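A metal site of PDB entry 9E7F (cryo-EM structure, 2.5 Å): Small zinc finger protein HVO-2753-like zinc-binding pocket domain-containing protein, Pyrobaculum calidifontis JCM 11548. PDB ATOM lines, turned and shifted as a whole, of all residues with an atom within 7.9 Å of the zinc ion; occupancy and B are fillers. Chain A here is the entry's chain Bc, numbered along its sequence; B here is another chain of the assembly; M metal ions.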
ATOM      1  N   ALA A  33      15.070 -23.517   8.789  1.00  0.00           N
ATOM      2  CA  ALA A  33      14.466 -24.763   8.357  1.00  0.00           C
ATOM      3  C   ALA A  33      14.458 -24.835   6.836  1.00  0.00           C
ATOM      4  O   ALA A  33      14.806 -23.866   6.156  1.00  0.00           O
ATOM      5  CB  ALA A  33      13.035 -24.890   8.893  1.00  0.00           C
ATOM      6  N   CYS A  34      14.091 -25.995   6.311  1.00  0.00           N
ATOM      7  CA  CYS A  34      14.010 -26.158   4.866  1.00  0.00           C
ATOM      8  C   CYS A  34      12.948 -25.214   4.298  1.00  0.00           C
ATOM      9  O   CYS A  34      11.854 -25.123   4.876  1.00  0.00           O
ATOM     10  CB  CYS A  34      13.674 -27.592   4.496  1.00  0.00           C
ATOM     11  SG  CYS A  34      13.332 -27.822   2.730  1.00  0.00           S
ATOM     12  N   PRO A  35      13.251 -24.464   3.237  1.00  0.00           N
ATOM     13  CA  PRO A  35      12.249 -23.541   2.689  1.00  0.00           C
ATOM     14  C   PRO A  35      10.996 -24.227   2.200  1.00  0.00           C
ATOM     15  O   PRO A  35       9.892 -23.695   2.371  1.00  0.00           O
ATOM     16  CB  PRO A  35      13.000 -22.852   1.546  1.00  0.00           C
ATOM     17  CG  PRO A  35      14.451 -23.075   1.849  1.00  0.00           C
ATOM     18  CD  PRO A  35      14.506 -24.419   2.485  1.00  0.00           C
ATOM     19  N   ASN A  36      11.133 -25.418   1.612  1.00  0.00           N
ATOM     20  CA  ASN A  36       9.959 -26.137   1.131  1.00  0.00           C
ATOM     21  C   ASN A  36       9.219 -26.804   2.279  1.00  0.00           C
ATOM     22  O   ASN A  36       8.044 -26.527   2.518  1.00  0.00           O
ATOM     23  CB  ASN A  36      10.370 -27.151   0.074  1.00  0.00           C
ATOM     24  CG  ASN A  36       9.425 -28.321  -0.008  1.00  0.00           C
ATOM     25  OD1 ASN A  36       8.314 -28.200  -0.507  1.00  0.00           O
ATOM     26  ND2 ASN A  36       9.855 -29.469   0.513  1.00  0.00           N
ATOM     27  N   CYS A  37       9.898 -27.668   3.024  1.00  0.00           N
ATOM     28  CA  CYS A  37       9.256 -28.347   4.137  1.00  0.00           C
ATOM     29  C   CYS A  37       9.144 -27.444   5.344  1.00  0.00           C
ATOM     30  O   CYS A  37       8.051 -27.156   5.825  1.00  0.00           O
ATOM     31  CB  CYS A  37      10.006 -29.620   4.522  1.00  0.00           C
ATOM     32  SG  CYS A  37      10.715 -30.546   3.155  1.00  0.00           S
ATOM     33  N   GLY A  38      10.282 -26.963   5.834  1.00  0.00           N
ATOM     34  CA  GLY A  38      10.366 -26.415   7.164  1.00  0.00           C
ATOM     35  C   GLY A  38      10.626 -27.445   8.235  1.00  0.00           C
ATOM     36  O   GLY A  38      10.591 -27.098   9.419  1.00  0.00           O
ATOM     37  N   LYS A  39      10.891 -28.691   7.855  1.00  0.00           N
ATOM     38  CA  LYS A  39      11.101 -29.773   8.810  1.00  0.00           C
ATOM     39  C   LYS A  39      12.561 -29.854   9.237  1.00  0.00           C
ATOM     40  O   LYS A  39      12.886 -29.704  10.420  1.00  0.00           O
ATOM     41  CB  LYS A  39      10.641 -31.099   8.210  1.00  0.00           C
ATOM     42  CG  LYS A  39       9.242 -31.046   7.621  1.00  0.00           C
ATOM     43  CD  LYS A  39       8.199 -31.409   8.672  1.00  0.00           C
ATOM     44  CE  LYS A  39       6.858 -31.703   8.032  1.00  0.00           C
ATOM     45  NZ  LYS A  39       6.900 -32.901   7.161  1.00  0.00           N
ATOM     46  N   THR A  40      13.459 -30.116   8.289  1.00  0.00           N
ATOM     47  CA  THR A  40      14.872 -30.243   8.608  1.00  0.00           C
ATOM     48  C   THR A  40      15.502 -28.864   8.772  1.00  0.00           C
ATOM     49  O   THR A  40      14.992 -27.852   8.286  1.00  0.00           O
ATOM     50  CB  THR A  40      15.592 -31.033   7.527  1.00  0.00           C
ATOM     51  OG1 THR A  40      14.714 -32.040   7.016  1.00  0.00           O
ATOM     52  CG2 THR A  40      16.832 -31.712   8.096  1.00  0.00           C
ATOM     53  N   ILE A  42      18.723 -26.298   8.311  1.00  0.00           N
ATOM     54  CA  ILE A  42      19.823 -26.034   7.399  1.00  0.00           C
ATOM     55  C   ILE A  42      20.807 -25.108   8.095  1.00  0.00           C
ATOM     56  O   ILE A  42      20.443 -23.991   8.498  1.00  0.00           O
ATOM     57  CB  ILE A  42      19.323 -25.408   6.095  1.00  0.00           C
ATOM     58  CG1 ILE A  42      18.615 -26.466   5.247  1.00  0.00           C
ATOM     59  CG2 ILE A  42      20.485 -24.822   5.316  1.00  0.00           C
ATOM     60  CD1 ILE A  42      19.427 -27.712   5.027  1.00  0.00           C
ATOM     61  N   ARG A  56      21.084 -29.189   0.351  1.00  0.00           N
ATOM     62  CA  ARG A  56      19.996 -30.063  -0.055  1.00  0.00           C
ATOM     63  C   ARG A  56      19.233 -30.527   1.174  1.00  0.00           C
ATOM     64  O   ARG A  56      19.838 -30.823   2.207  1.00  0.00           O
ATOM     65  CB  ARG A  56      20.531 -31.275  -0.841  1.00  0.00           C
ATOM     66  CG  ARG A  56      19.477 -32.016  -1.619  1.00  0.00           C
ATOM     67  CD  ARG A  56      20.027 -33.315  -2.158  1.00  0.00           C
ATOM     68  NE  ARG A  56      19.458 -34.478  -1.497  1.00  0.00           N
ATOM     69  CZ  ARG A  56      18.283 -35.011  -1.803  1.00  0.00           C
ATOM     70  NH1 ARG A  56      17.524 -34.504  -2.758  1.00  0.00           N
ATOM     71  NH2 ARG A  56      17.861 -36.076  -1.130  1.00  0.00           N
ATOM     72  N   CYS A  57      17.916 -30.578   1.063  1.00  0.00           N
ATOM     73  CA  CYS A  57      17.110 -31.098   2.148  1.00  0.00           C
ATOM     74  C   CYS A  57      17.284 -32.612   2.235  1.00  0.00           C
ATOM     75  O   CYS A  57      17.170 -33.300   1.223  1.00  0.00           O
ATOM     76  CB  CYS A  57      15.635 -30.767   1.943  1.00  0.00           C
ATOM     77  SG  CYS A  57      14.552 -31.352   3.278  1.00  0.00           S
ATOM     78  N   PRO A  58      17.595 -33.160   3.411  1.00  0.00           N
ATOM     79  CA  PRO A  58      17.627 -34.623   3.545  1.00  0.00           C
ATOM     80  C   PRO A  58      16.264 -35.267   3.374  1.00  0.00           C
ATOM     81  O   PRO A  58      16.207 -36.455   3.033  1.00  0.00           O
ATOM     82  CB  PRO A  58      18.189 -34.838   4.958  1.00  0.00           C
ATOM     83  CG  PRO A  58      18.570 -33.514   5.481  1.00  0.00           C
ATOM     84  CD  PRO A  58      17.926 -32.461   4.657  1.00  0.00           C
ATOM     85  N   GLU A  59      15.176 -34.534   3.595  1.00  0.00           N
ATOM     86  CA  GLU A  59      13.841 -35.108   3.504  1.00  0.00           C
ATOM     87  C   GLU A  59      13.193 -34.903   2.141  1.00  0.00           C
ATOM     88  O   GLU A  59      12.659 -35.851   1.572  1.00  0.00           O
ATOM     89  CB  GLU A  59      12.947 -34.499   4.589  1.00  0.00           C
ATOM     90  CG  GLU A  59      13.519 -34.618   5.979  1.00  0.00           C
ATOM     91  CD  GLU A  59      12.493 -34.276   7.044  1.00  0.00           C
ATOM     92  OE1 GLU A  59      11.402 -33.794   6.690  1.00  0.00           O
ATOM     93  OE2 GLU A  59      12.789 -34.486   8.243  1.00  0.00           O
ATOM     94  N   CYS A  60      13.211 -33.677   1.625  1.00  0.00           N
ATOM     95  CA  CYS A  60      12.677 -33.391   0.293  1.00  0.00           C
ATOM     96  C   CYS A  60      13.829 -33.059  -0.635  1.00  0.00           C
ATOM     97  O   CYS A  60      14.951 -32.808  -0.199  1.00  0.00           O
ATOM     98  CB  CYS A  60      11.678 -32.233   0.336  1.00  0.00           C
ATOM     99  SG  CYS A  60      12.442 -30.606   0.162  1.00  0.00           S
ATOM    100  N   GLY A  61      13.547 -33.023  -1.926  1.00  0.00           N
ATOM    101  CA  GLY A  61      14.615 -32.867  -2.895  1.00  0.00           C
ATOM    102  C   GLY A  61      15.057 -31.447  -3.143  1.00  0.00           C
ATOM    103  O   GLY A  61      15.797 -31.202  -4.098  1.00  0.00           O
ATOM    104  N   PHE A  62      14.635 -30.507  -2.300  1.00  0.00           N
ATOM    105  CA  PHE A  62      14.920 -29.095  -2.539  1.00  0.00           C
ATOM    106  C   PHE A  62      16.403 -28.817  -2.356  1.00  0.00           C
ATOM    107  O   PHE A  62      17.020 -29.274  -1.396  1.00  0.00           O
ATOM    108  CB  PHE A  62      14.098 -28.215  -1.595  1.00  0.00           C
ATOM    109  CG  PHE A  62      14.404 -26.746  -1.708  1.00  0.00           C
ATOM    110  CD1 PHE A  62      15.246 -26.131  -0.799  1.00  0.00           C
ATOM    111  CD2 PHE A  62      13.844 -25.996  -2.709  1.00  0.00           C
ATOM    112  CE1 PHE A  62      15.527 -24.786  -0.900  1.00  0.00           C
ATOM    113  CE2 PHE A  62      14.125 -24.651  -2.810  1.00  0.00           C
ATOM    114  CZ  PHE A  62      14.969 -24.050  -1.903  1.00  0.00           C
ATOM    115  N   VAL A  63      16.962 -28.062  -3.297  1.00  0.00           N
ATOM    116  CA  VAL A  63      18.354 -27.610  -3.235  1.00  0.00           C
ATOM    117  C   VAL A  63      18.361 -26.105  -3.413  1.00  0.00           C
ATOM    118  O   VAL A  63      17.640 -25.567  -4.256  1.00  0.00           O
ATOM    119  CB  VAL A  63      19.221 -28.301  -4.303  1.00  0.00           C
ATOM    120  CG1 VAL A  63      19.169 -29.802  -4.121  1.00  0.00           C
ATOM    121  CG2 VAL A  63      18.743 -27.941  -5.702  1.00  0.00           C
ATOM    122  N   LYS B  63       6.309 -19.681   1.707  1.00  0.00           N
ATOM    123  CA  LYS B  63       6.418 -20.648   2.791  1.00  0.00           C
ATOM    124  C   LYS B  63       7.464 -20.222   3.809  1.00  0.00           C
ATOM    125  O   LYS B  63       7.252 -20.336   5.016  1.00  0.00           O
ATOM    126  CB  LYS B  63       6.741 -22.033   2.223  1.00  0.00           C
ATOM    127  CG  LYS B  63       5.531 -22.907   1.948  1.00  0.00           C
ATOM    128  CD  LYS B  63       5.926 -24.342   1.653  1.00  0.00           C
ATOM    129  CE  LYS B  63       6.029 -24.599   0.164  1.00  0.00           C
ATOM    130  NZ  LYS B  63       6.765 -25.856  -0.168  1.00  0.00           N
HETATM  131 ZN    ZN M   1      12.836 -30.064   2.380  1.00  0.00          ZN
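ND2 of Asn 36 touches the zinc ion, 3.6 Å away.
Within 4 Å of the zinc ion: Cys 34, Asn 36, Cys 37, Cys 57 and Cys 60.
The side-chain amide nitrogen of Asn 36 sits close to the side-chain sulfur of Cys 37, at 3.0 Å.
SG of Cys 60 lies close to ND2 of Asn 36 (2.8 Å).
The backbone NH (N) of Phe 62 lies close to the side-chain sulfur (SG) of Cys 60.
SG of Cys 34 lies close to N of Asn 36 (3.4 Å).
N of Cys 34 sits at hydrogen-bond distance from O of Thr 40.
The backbone NH (N) of Cys 57 is in hydrogen-bond range of the backbone carbonyl oxygen (O) of Phe 62, at 2.9 Å.
The side-chain sulfur (SG) of Cys 57 lies close to the backbone NH (N) of Glu 59.
OD1 of Asn 36 is in hydrogen-bond range of NZ of Lys 63 of chain B (2.8 Å).
SG of Cys 37 is bound to the zinc ion (2.3 Å).
The zinc ion is bound by SG of Cys 60 (2.3 Å).
SG of Cys 34 binds the zinc ion, at 2.3 Å.
SG of Cys 57 binds the zinc ion (2.3 Å).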
